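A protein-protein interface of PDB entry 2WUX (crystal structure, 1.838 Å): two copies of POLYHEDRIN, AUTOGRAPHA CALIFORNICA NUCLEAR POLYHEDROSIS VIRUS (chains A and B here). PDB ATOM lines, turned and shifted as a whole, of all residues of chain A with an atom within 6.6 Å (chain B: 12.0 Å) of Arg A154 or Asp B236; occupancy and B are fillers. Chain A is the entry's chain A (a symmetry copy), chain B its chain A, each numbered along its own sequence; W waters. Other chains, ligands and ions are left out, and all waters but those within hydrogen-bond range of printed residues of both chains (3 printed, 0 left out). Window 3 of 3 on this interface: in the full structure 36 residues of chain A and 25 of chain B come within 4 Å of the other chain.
Water W3 lies within hydrogen-bond range of the backbone carbonyl oxygen of Glu B232, the backbone carbonyl oxygen of Arg A154 and the backbone NH of Ala B234. Water W1 lies within hydrogen-bond range of the backbone carbonyl oxygen (O) of Val A156 (2.8 Å) and the backbone NH (N) of Glu B232 (2.9 Å). Water W2 lies within hydrogen-bond range of NE2 of His A150 and N of Asp B112.
Hydrophobic or aromatic side chains of chain A within 4 Å of the printed part of chain B: His A150, Val A152, Ile A153 and Val A156. Printed residues of chain B that touch a printed residue of chain A: Lys B65, Asp B112, Phe B233, Ala B234, Pro B235 and Asp B236. Hydrophobic or aromatic side chains of chain B within 4 Å of the printed part of chain A: Phe B233 and Pro B235. Along chain B the printed residues that touch a printed residue of chain A span positions 65 to 236. Among the printed residues, 11 pairs touch across the chains. Among the printed residues, Asp or Glu carboxylates within 4 Å of a Lys or Arg side-chain nitrogen of the other chain: Arg A154 with Asp B236 (2.9 Å).
No position is printed for both chains.
Among the printed residues, merely in contact across the chains: Ile A153 with Ala B234 (3.2 Å), His A150 with Pro B235 (3.5 Å), Val A152 with Pro B235 (3.5 Å), His A150 with Phe B233 (3.6 Å), Arg A154 with Pro B235 (3.8 Å), Val A156 with Lys B65 (3.8 Å) and Ile A153 with Phe B233 (3.9 Å).
No residue of chain B comes within 4 Å of Thr A82. Of chain B, only Pro B235 and Asp B236 come within 4 Å of Val A152. Printed residues of chain B within 4 Å of Ile A153: Phe B233 and Ala B234. Arg A154 touches just these residues of chain B: Ala B234, Pro B235 and Asp B236. Ile A155 touches none of the printed residues of chain B. Val A156 touches just one residue of chain B: Lys B65 (3.8 Å). Of the printed residues of chain A, Lys B65 touches Val A156. Lys B231 touches none of the printed residues of chain A. Printed residues of chain A within 4 Å of Phe B233: His A150 (3.6 Å) and Ile A153 (3.9 Å). Of the printed residues of chain A, Pro B235 touches His A150, Val A152 and Arg A154. Of the printed residues of chain A, Asp B236 touches Val A152 and Arg A154. The nearest residue of chain B that does not touch Arg A154 is Glu B232 (5.0 Å). The nearest printed residue of chain A that does not touch Asp B236 is Ile A153 (4.002 Å).
OE1 of Glu B232 is in salt-bridge range of NZ of Lys B65 (2.7 Å). The backbone NH (N) of Phe B233 lies within hydrogen-bond range of the backbone carbonyl oxygen (O) of Asp B112 (2.8 Å). The side-chain carboxylate (OD2) of Asp A81 lies within salt-bridge range of the guanidinium group (NH1) of Arg A154 (2.8 Å). The backbone carbonyl oxygen of Val B230 lies within hydrogen-bond range of the backbone NH of Lys B65 (2.6 Å). The backbone NH of Met A83 lies within hydrogen-bond range of the backbone carbonyl oxygen of Ile A153 (2.9 Å).
The side-chain carboxylate of Asp B112 is in hydrogen-bond range of a ring nitrogen (NE2) of His A150, at 3.4 Å. O of Ala B234 sits at hydrogen-bond distance from N of Arg A154 (2.8 Å). The side-chain carboxylate (OD1) of Asp B236 is in salt-bridge range of the guanidinium group (NH2) of Arg A154 (2.9 Å). The backbone carbonyl oxygen (O) of Val A152 sits at hydrogen-bond distance from the backbone NH (N) of Asp B236 (3.2 Å).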
ATOM      1  N   LYS A  79      24.532 -39.896  19.403  1.00  0.00           N
ATOM      2  CA  LYS A  79      25.067 -39.504  18.101  1.00  0.00           C
ATOM      3  C   LYS A  79      26.363 -38.715  18.249  1.00  0.00           C
ATOM      4  O   LYS A  79      26.597 -38.086  19.284  1.00  0.00           O
ATOM      5  CB  LYS A  79      24.030 -38.700  17.309  1.00  0.00           C
ATOM      6  CG  LYS A  79      22.663 -39.372  17.233  1.00  0.00           C
ATOM      7  CD  LYS A  79      22.732 -40.745  16.572  1.00  0.00           C
ATOM      8  CE  LYS A  79      21.364 -41.429  16.517  1.00  0.00           C
ATOM      9  NZ  LYS A  79      20.922 -42.007  17.829  1.00  0.00           N
ATOM     10  N   PRO A  80      27.225 -38.753  17.214  1.00  0.00           N
ATOM     11  CA  PRO A  80      28.505 -38.047  17.341  1.00  0.00           C
ATOM     12  C   PRO A  80      28.282 -36.567  17.640  1.00  0.00           C
ATOM     13  O   PRO A  80      27.282 -35.997  17.211  1.00  0.00           O
ATOM     14  CB  PRO A  80      29.141 -38.221  15.959  1.00  0.00           C
ATOM     15  CG  PRO A  80      28.559 -39.492  15.439  1.00  0.00           C
ATOM     16  CD  PRO A  80      27.153 -39.560  15.983  1.00  0.00           C
ATOM     17  N   ASP A  81      29.197 -35.984  18.405  1.00  0.00           N
ATOM     18  CA  ASP A  81      29.148 -34.571  18.774  1.00  0.00           C
ATOM     19  C   ASP A  81      27.944 -34.171  19.626  1.00  0.00           C
ATOM     20  O   ASP A  81      27.656 -32.978  19.768  1.00  0.00           O
ATOM     21  CB  ASP A  81      29.251 -33.660  17.539  1.00  0.00           C
ATOM     22  CG  ASP A  81      29.908 -32.324  17.873  1.00  0.00           C
ATOM     23  OD1 ASP A  81      30.758 -32.307  18.785  1.00  0.00           O
ATOM     24  OD2 ASP A  81      29.567 -31.303  17.254  1.00  0.00           O
ATOM     25  N   THR A  82      27.259 -35.156  20.210  1.00  0.00           N
ATOM     26  CA  THR A  82      26.190 -34.871  21.148  1.00  0.00           C
ATOM     27  C   THR A  82      26.349 -35.641  22.446  1.00  0.00           C
ATOM     28  O   THR A  82      27.163 -36.565  22.556  1.00  0.00           O
ATOM     29  CB  THR A  82      24.788 -35.210  20.571  1.00  0.00           C
ATOM     30  OG1 THR A  82      24.615 -36.627  20.547  1.00  0.00           O
ATOM     31  CG2 THR A  82      24.631 -34.647  19.156  1.00  0.00           C
ATOM     32  N   MET A  83      25.552 -35.257  23.434  1.00  0.00           N
ATOM     33  CA  MET A  83      25.451 -36.003  24.680  1.00  0.00           C
ATOM     34  C   MET A  83      23.988 -36.076  25.072  1.00  0.00           C
ATOM     35  O   MET A  83      23.234 -35.130  24.847  1.00  0.00           O
ATOM     36  CB  MET A  83      26.219 -35.299  25.795  1.00  0.00           C
ATOM     37  CG  MET A  83      27.535 -34.687  25.341  1.00  0.00           C
ATOM     38  SD  MET A  83      28.267 -33.645  26.620  1.00  0.00           S
ATOM     39  CE  MET A  83      28.519 -34.850  27.872  1.00  0.00           C
ATOM     40  N   HIS A 150      17.221 -30.070  28.446  1.00  0.00           N
ATOM     41  CA  HIS A 150      17.218 -30.672  27.133  1.00  0.00           C
ATOM     42  C   HIS A 150      17.563 -32.131  27.238  1.00  0.00           C
ATOM     43  O   HIS A 150      18.436 -32.515  28.024  1.00  0.00           O
ATOM     44  CB  HIS A 150      18.262 -30.015  26.238  1.00  0.00           C
ATOM     45  CG  HIS A 150      18.085 -28.545  26.104  1.00  0.00           C
ATOM     46  ND1 HIS A 150      16.995 -27.989  25.467  1.00  0.00           N
ATOM     47  CD2 HIS A 150      18.853 -27.510  26.524  1.00  0.00           C
ATOM     48  CE1 HIS A 150      17.105 -26.670  25.498  1.00  0.00           C
ATOM     49  NE2 HIS A 150      18.222 -26.356  26.135  1.00  0.00           N
ATOM     50  N   VAL A 152      18.909 -33.770  24.701  1.00  0.00           N
ATOM     51  CA  VAL A 152      20.091 -33.953  23.860  1.00  0.00           C
ATOM     52  C   VAL A 152      20.786 -32.605  23.688  1.00  0.00           C
ATOM     53  O   VAL A 152      20.146 -31.614  23.347  1.00  0.00           O
ATOM     54  CB  VAL A 152      19.712 -34.497  22.453  1.00  0.00           C
ATOM     55  CG1 VAL A 152      20.958 -34.917  21.668  1.00  0.00           C
ATOM     56  CG2 VAL A 152      18.729 -35.667  22.562  1.00  0.00           C
ATOM     57  N   ILE A 153      22.087 -32.564  23.949  1.00  0.00           N
ATOM     58  CA  ILE A 153      22.842 -31.335  23.764  1.00  0.00           C
ATOM     59  C   ILE A 153      24.053 -31.580  22.868  1.00  0.00           C
ATOM     60  O   ILE A 153      24.406 -32.730  22.572  1.00  0.00           O
ATOM     61  CB  ILE A 153      23.279 -30.717  25.112  1.00  0.00           C
ATOM     62  CG1 ILE A 153      24.270 -31.641  25.820  1.00  0.00           C
ATOM     63  CG2 ILE A 153      22.038 -30.399  25.983  1.00  0.00           C
ATOM     64  CD1 ILE A 153      24.873 -31.055  27.086  1.00  0.00           C
ATOM     65  N   ARG A 154      24.669 -30.496  22.407  1.00  0.00           N
ATOM     66  CA  ARG A 154      25.901 -30.587  21.628  1.00  0.00           C
ATOM     67  C   ARG A 154      27.082 -30.647  22.580  1.00  0.00           C
ATOM     68  O   ARG A 154      27.019 -30.117  23.687  1.00  0.00           O
ATOM     69  CB  ARG A 154      26.068 -29.357  20.731  1.00  0.00           C
ATOM     70  CG  ARG A 154      24.966 -29.180  19.729  1.00  0.00           C
ATOM     71  CD  ARG A 154      24.818 -30.390  18.843  1.00  0.00           C
ATOM     72  NE  ARG A 154      25.974 -30.564  17.974  1.00  0.00           N
ATOM     73  CZ  ARG A 154      25.918 -31.063  16.747  1.00  0.00           C
ATOM     74  NH1 ARG A 154      27.027 -31.186  16.023  1.00  0.00           N
ATOM     75  NH2 ARG A 154      24.752 -31.436  16.242  1.00  0.00           N
ATOM     76  N   ILE A 155      28.165 -31.273  22.146  1.00  0.00           N
ATOM     77  CA  ILE A 155      29.369 -31.343  22.970  1.00  0.00           C
ATOM     78  C   ILE A 155      30.087 -29.998  22.934  1.00  0.00           C
ATOM     79  O   ILE A 155      30.459 -29.522  21.865  1.00  0.00           O
ATOM     80  CB  ILE A 155      30.331 -32.468  22.485  1.00  0.00           C
ATOM     81  CG1 ILE A 155      29.681 -33.841  22.661  1.00  0.00           C
ATOM     82  CG2 ILE A 155      31.643 -32.415  23.259  1.00  0.00           C
ATOM     83  CD1 ILE A 155      30.502 -35.013  22.066  1.00  0.00           C
ATOM     84  N   VAL A 156      30.275 -29.385  24.099  1.00  0.00           N
ATOM     85  CA  VAL A 156      31.004 -28.112  24.199  1.00  0.00           C
ATOM     86  C   VAL A 156      31.943 -28.124  25.415  1.00  0.00           C
ATOM     87  O   VAL A 156      31.486 -28.030  26.561  1.00  0.00           O
ATOM     88  CB  VAL A 156      30.031 -26.918  24.325  1.00  0.00           C
ATOM     89  CG1 VAL A 156      30.795 -25.593  24.444  1.00  0.00           C
ATOM     90  CG2 VAL A 156      29.062 -26.880  23.144  1.00  0.00           C
ATOM     91  N   PRO B  63      37.300 -28.301  31.574  1.00  0.00           N
ATOM     92  CA  PRO B  63      35.966 -28.198  30.966  1.00  0.00           C
ATOM     93  C   PRO B  63      35.373 -26.792  31.048  1.00  0.00           C
ATOM     94  O   PRO B  63      35.715 -26.005  31.933  1.00  0.00           O
ATOM     95  CB  PRO B  63      35.128 -29.165  31.796  1.00  0.00           C
ATOM     96  CG  PRO B  63      36.141 -30.214  32.275  1.00  0.00           C
ATOM     97  CD  PRO B  63      37.413 -29.445  32.494  1.00  0.00           C
ATOM     98  N   GLY B  64      34.467 -26.497  30.125  1.00  0.00           N
ATOM     99  CA  GLY B  64      33.783 -25.219  30.101  1.00  0.00           C
ATOM    100  C   GLY B  64      34.492 -24.254  29.185  1.00  0.00           C
ATOM    101  O   GLY B  64      35.691 -24.374  28.966  1.00  0.00           O
ATOM    102  N   LYS B  65      33.743 -23.294  28.657  1.00  0.00           N
ATOM    103  CA  LYS B  65      34.288 -22.306  27.745  1.00  0.00           C
ATOM    104  C   LYS B  65      35.020 -21.253  28.545  1.00  0.00           C
ATOM    105  O   LYS B  65      34.688 -21.016  29.699  1.00  0.00           O
ATOM    106  CB  LYS B  65      33.155 -21.630  26.966  1.00  0.00           C
ATOM    107  CG  LYS B  65      32.216 -22.591  26.253  1.00  0.00           C
ATOM    108  CD  LYS B  65      31.427 -21.879  25.139  1.00  0.00           C
ATOM    109  CE  LYS B  65      30.692 -20.654  25.648  1.00  0.00           C
ATOM    110  NZ  LYS B  65      29.625 -20.215  24.674  1.00  0.00           N
ATOM    111  N   VAL B 110      21.949 -17.379  24.112  1.00  0.00           N
ATOM    112  CA  VAL B 110      20.950 -18.111  23.328  1.00  0.00           C
ATOM    113  C   VAL B 110      20.591 -19.465  23.928  1.00  0.00           C
ATOM    114  O   VAL B 110      19.536 -20.025  23.621  1.00  0.00           O
ATOM    115  CB  VAL B 110      21.405 -18.317  21.858  1.00  0.00           C
ATOM    116  CG1 VAL B 110      21.660 -16.990  21.182  1.00  0.00           C
ATOM    117  CG2 VAL B 110      22.643 -19.170  21.796  1.00  0.00           C
ATOM    118  N   ASN B 111      21.456 -19.979  24.798  1.00  0.00           N
ATOM    119  CA  ASN B 111      21.235 -21.298  25.386  1.00  0.00           C
ATOM    120  C   ASN B 111      21.286 -21.272  26.904  1.00  0.00           C
ATOM    121  O   ASN B 111      21.870 -20.378  27.479  1.00  0.00           O
ATOM    122  CB  ASN B 111      22.305 -22.271  24.887  1.00  0.00           C
ATOM    123  CG  ASN B 111      22.248 -22.475  23.389  1.00  0.00           C
ATOM    124  OD1 ASN B 111      21.175 -22.677  22.827  1.00  0.00           O
ATOM    125  ND2 ASN B 111      23.400 -22.427  22.739  1.00  0.00           N
ATOM    126  N   ASP B 112      20.681 -22.263  27.547  1.00  0.00           N
ATOM    127  CA  ASP B 112      20.907 -22.455  28.970  1.00  0.00           C
ATOM    128  C   ASP B 112      22.408 -22.561  29.187  1.00  0.00           C
ATOM    129  O   ASP B 112      23.105 -23.295  28.475  1.00  0.00           O
ATOM    130  CB  ASP B 112      20.248 -23.741  29.464  1.00  0.00           C
ATOM    131  CG  ASP B 112      18.742 -23.737  29.270  1.00  0.00           C
ATOM    132  OD1 ASP B 112      18.157 -22.637  29.184  1.00  0.00           O
ATOM    133  OD2 ASP B 112      18.146 -24.835  29.211  1.00  0.00           O
ATOM    134  N   GLN B 113      22.912 -21.817  30.158  1.00  0.00           N
ATOM    135  CA  GLN B 113      24.317 -21.970  30.531  1.00  0.00           C
ATOM    136  C   GLN B 113      24.501 -21.710  32.013  1.00  0.00           C
ATOM    137  O   GLN B 113      23.629 -21.141  32.678  1.00  0.00           O
ATOM    138  CB  GLN B 113      25.211 -21.036  29.712  1.00  0.00           C
ATOM    139  CG  GLN B 113      24.861 -19.553  29.845  1.00  0.00           C
ATOM    140  CD  GLN B 113      25.891 -18.658  29.172  1.00  0.00           C
ATOM    141  OE1 GLN B 113      26.345 -17.660  29.751  1.00  0.00           O
ATOM    142  NE2 GLN B 113      26.282 -19.019  27.956  1.00  0.00           N
ATOM    143  N   GLU B 114      25.645 -22.148  32.515  1.00  0.00           N
ATOM    144  CA  GLU B 114      26.001 -21.951  33.896  1.00  0.00           C
ATOM    145  C   GLU B 114      27.352 -21.257  33.951  1.00  0.00           C
ATOM    146  O   GLU B 114      28.313 -21.703  33.326  1.00  0.00           O
ATOM    147  CB  GLU B 114      26.048 -23.311  34.591  1.00  0.00           C
ATOM    148  CG  GLU B 114      26.864 -23.352  35.869  1.00  0.00           C
ATOM    149  CD  GLU B 114      26.939 -24.751  36.454  1.00  0.00           C
ATOM    150  OE1 GLU B 114      26.176 -25.629  36.002  1.00  0.00           O
ATOM    151  OE2 GLU B 114      27.763 -24.970  37.367  1.00  0.00           O
ATOM    152  N   VAL B 230      32.371 -20.784  31.437  1.00  0.00           N
ATOM    153  CA  VAL B 230      30.973 -20.992  31.102  1.00  0.00           C
ATOM    154  C   VAL B 230      30.709 -22.412  30.591  1.00  0.00           C
ATOM    155  O   VAL B 230      31.376 -22.913  29.682  1.00  0.00           O
ATOM    156  CB  VAL B 230      30.474 -19.961  30.063  1.00  0.00           C
ATOM    157  CG1 VAL B 230      28.973 -20.100  29.857  1.00  0.00           C
ATOM    158  CG2 VAL B 230      30.834 -18.543  30.502  1.00  0.00           C
ATOM    159  N   LYS B 231      29.715 -23.054  31.183  1.00  0.00           N
ATOM    160  CA  LYS B 231      29.297 -24.374  30.754  1.00  0.00           C
ATOM    161  C   LYS B 231      28.006 -24.194  29.969  1.00  0.00           C
ATOM    162  O   LYS B 231      26.990 -23.767  30.531  1.00  0.00           O
ATOM    163  CB  LYS B 231      29.079 -25.221  32.003  1.00  0.00           C
ATOM    164  CG  LYS B 231      28.641 -26.627  31.779  1.00  0.00           C
ATOM    165  CD  LYS B 231      28.232 -27.245  33.127  1.00  0.00           C
ATOM    166  CE  LYS B 231      29.347 -27.140  34.163  1.00  0.00           C
ATOM    167  NZ  LYS B 231      28.967 -27.804  35.459  1.00  0.00           N
ATOM    168  N   GLU B 232      28.047 -24.487  28.669  1.00  0.00           N
ATOM    169  CA  GLU B 232      26.913 -24.227  27.783  1.00  0.00           C
ATOM    170  C   GLU B 232      26.110 -25.501  27.500  1.00  0.00           C
ATOM    171  O   GLU B 232      26.680 -26.540  27.196  1.00  0.00           O
ATOM    172  CB  GLU B 232      27.401 -23.621  26.459  1.00  0.00           C
ATOM    173  CG  GLU B 232      26.274 -23.230  25.482  1.00  0.00           C
ATOM    174  CD  GLU B 232      26.770 -22.376  24.301  1.00  0.00           C
ATOM    175  OE1 GLU B 232      28.001 -22.286  24.074  1.00  0.00           O
ATOM    176  OE2 GLU B 232      25.926 -21.776  23.606  1.00  0.00           O
ATOM    177  N   PHE B 233      24.787 -25.407  27.603  1.00  0.00           N
ATOM    178  CA  PHE B 233      23.905 -26.523  27.299  1.00  0.00           C
ATOM    179  C   PHE B 233      23.096 -26.176  26.062  1.00  0.00           C
ATOM    180  O   PHE B 233      21.944 -25.745  26.153  1.00  0.00           O
ATOM    181  CB  PHE B 233      22.994 -26.852  28.491  1.00  0.00           C
ATOM    182  CG  PHE B 233      23.749 -27.291  29.722  1.00  0.00           C
ATOM    183  CD1 PHE B 233      23.964 -28.631  29.981  1.00  0.00           C
ATOM    184  CD2 PHE B 233      24.270 -26.352  30.609  1.00  0.00           C
ATOM    185  CE1 PHE B 233      24.661 -29.040  31.121  1.00  0.00           C
ATOM    186  CE2 PHE B 233      24.970 -26.745  31.745  1.00  0.00           C
ATOM    187  CZ  PHE B 233      25.168 -28.094  32.006  1.00  0.00           C
ATOM    188  N   ALA B 234      23.722 -26.355  24.904  1.00  0.00           N
ATOM    189  CA  ALA B 234      23.118 -26.031  23.618  1.00  0.00           C
ATOM    190  C   ALA B 234      22.396 -27.261  23.059  1.00  0.00           C
ATOM    191  O   ALA B 234      23.014 -28.314  22.869  1.00  0.00           O
ATOM    192  CB  ALA B 234      24.203 -25.560  22.643  1.00  0.00           C
ATOM    193  N   PRO B 235      21.090 -27.141  22.792  1.00  0.00           N
ATOM    194  CA  PRO B 235      20.370 -28.317  22.294  1.00  0.00           C
ATOM    195  C   PRO B 235      20.877 -28.764  20.921  1.00  0.00           C
ATOM    196  O   PRO B 235      21.427 -27.971  20.140  1.00  0.00           O
ATOM    197  CB  PRO B 235      18.924 -27.831  22.153  1.00  0.00           C
ATOM    198  CG  PRO B 235      18.915 -26.390  22.554  1.00  0.00           C
ATOM    199  CD  PRO B 235      20.303 -25.903  22.667  1.00  0.00           C
ATOM    200  N   ASP B 236      20.702 -30.044  20.638  1.00  0.00           N
ATOM    201  CA  ASP B 236      20.978 -30.559  19.305  1.00  0.00           C
ATOM    202  C   ASP B 236      19.801 -30.149  18.441  1.00  0.00           C
ATOM    203  O   ASP B 236      18.870 -30.926  18.229  1.00  0.00           O
ATOM    204  CB  ASP B 236      21.113 -32.086  19.342  1.00  0.00           C
ATOM    205  CG  ASP B 236      21.314 -32.688  17.965  1.00  0.00           C
ATOM    206  OD1 ASP B 236      22.121 -32.127  17.193  1.00  0.00           O
ATOM    207  OD2 ASP B 236      20.669 -33.722  17.663  1.00  0.00           O
ATOM    208  N   ALA B 237      19.843 -28.910  17.968  1.00  0.00           N
ATOM    209  CA  ALA B 237      18.740 -28.310  17.235  1.00  0.00           C
ATOM    210  C   ALA B 237      19.256 -27.201  16.327  1.00  0.00           C
ATOM    211  O   ALA B 237      20.062 -26.379  16.739  1.00  0.00           O
ATOM    212  CB  ALA B 237      17.701 -27.750  18.213  1.00  0.00           C
ATOM    213  N   PRO B 238      18.780 -27.162  15.081  1.00  0.00           N
ATOM    214  CA  PRO B 238      19.306 -26.154  14.160  1.00  0.00           C
ATOM    215  C   PRO B 238      18.648 -24.797  14.375  1.00  0.00           C
ATOM    216  O   PRO B 238      17.618 -24.698  15.053  1.00  0.00           O
ATOM    217  CB  PRO B 238      18.891 -26.697  12.786  1.00  0.00           C
ATOM    218  CG  PRO B 238      17.624 -27.482  13.065  1.00  0.00           C
ATOM    219  CD  PRO B 238      17.737 -28.016  14.470  1.00  0.00           C
ATOM    220  N   LEU B 239      19.246 -23.769  13.790  1.00  0.00           N
ATOM    221  CA  LEU B 239      18.584 -22.471  13.659  1.00  0.00           C
ATOM    222  C   LEU B 239      17.882 -22.404  12.304  1.00  0.00           C
ATOM    223  O   LEU B 239      18.520 -22.570  11.270  1.00  0.00           O
ATOM    224  CB  LEU B 239      19.602 -21.339  13.751  1.00  0.00           C
ATOM    225  CG  LEU B 239      19.042 -19.936  13.523  1.00  0.00           C
ATOM    226  CD1 LEU B 239      18.059 -19.541  14.628  1.00  0.00           C
ATOM    227  CD2 LEU B 239      20.187 -18.910  13.376  1.00  0.00           C
ATOM    228  N   PHE B 240      16.578 -22.143  12.305  1.00  0.00           N
ATOM    229  CA  PHE B 240      15.819 -22.015  11.063  1.00  0.00           C
ATOM    230  C   PHE B 240      15.413 -20.573  10.806  1.00  0.00           C
ATOM    231  O   PHE B 240      15.167 -19.825  11.739  1.00  0.00           O
ATOM    232  CB  PHE B 240      14.512 -22.798  11.151  1.00  0.00           C
ATOM    233  CG  PHE B 240      14.682 -24.295  11.098  1.00  0.00           C
ATOM    234  CD1 PHE B 240      13.865 -25.116  11.855  1.00  0.00           C
ATOM    235  CD2 PHE B 240      15.632 -24.875  10.277  1.00  0.00           C
ATOM    236  CE1 PHE B 240      13.989 -26.509  11.791  1.00  0.00           C
ATOM    237  CE2 PHE B 240      15.766 -26.271  10.219  1.00  0.00           C
ATOM    238  CZ  PHE B 240      14.943 -27.077  10.979  1.00  0.00           C
ATOM    239  N   TYR B 245       9.718 -24.865   9.221  1.00  0.00           N
ATOM    240  CA  TYR B 245       8.968 -25.857   8.444  1.00  0.00           C
ATOM    241  C   TYR B 245       7.887 -25.300   7.504  1.00  0.00           C
ATOM    242  O   TYR B 245       7.135 -26.076   6.903  1.00  0.00           O
ATOM    243  CB  TYR B 245       8.370 -26.943   9.349  1.00  0.00           C
ATOM    244  CG  TYR B 245       9.425 -27.719  10.095  1.00  0.00           C
ATOM    245  CD1 TYR B 245       9.667 -27.473  11.437  1.00  0.00           C
ATOM    246  CD2 TYR B 245      10.208 -28.672   9.447  1.00  0.00           C
ATOM    247  CE1 TYR B 245      10.631 -28.176  12.135  1.00  0.00           C
ATOM    248  CE2 TYR B 245      11.200 -29.372  10.135  1.00  0.00           C
ATOM    249  CZ  TYR B 245      11.398 -29.113  11.480  1.00  0.00           C
ATOM    250  OH  TYR B 245      12.359 -29.786  12.188  1.00  0.00           O
ATOM    251  OXT TYR B 245       7.721 -24.094   7.312  1.00  0.00           O
HETATM  252  O   HOH W   1      30.467 -25.928  28.029  1.00  0.00           O
HETATM  253  O   HOH W   2      18.540 -23.581  25.797  1.00  0.00           O
HETATM  254  O   HOH W   3      26.088 -27.891  24.940  1.00  0.00           O
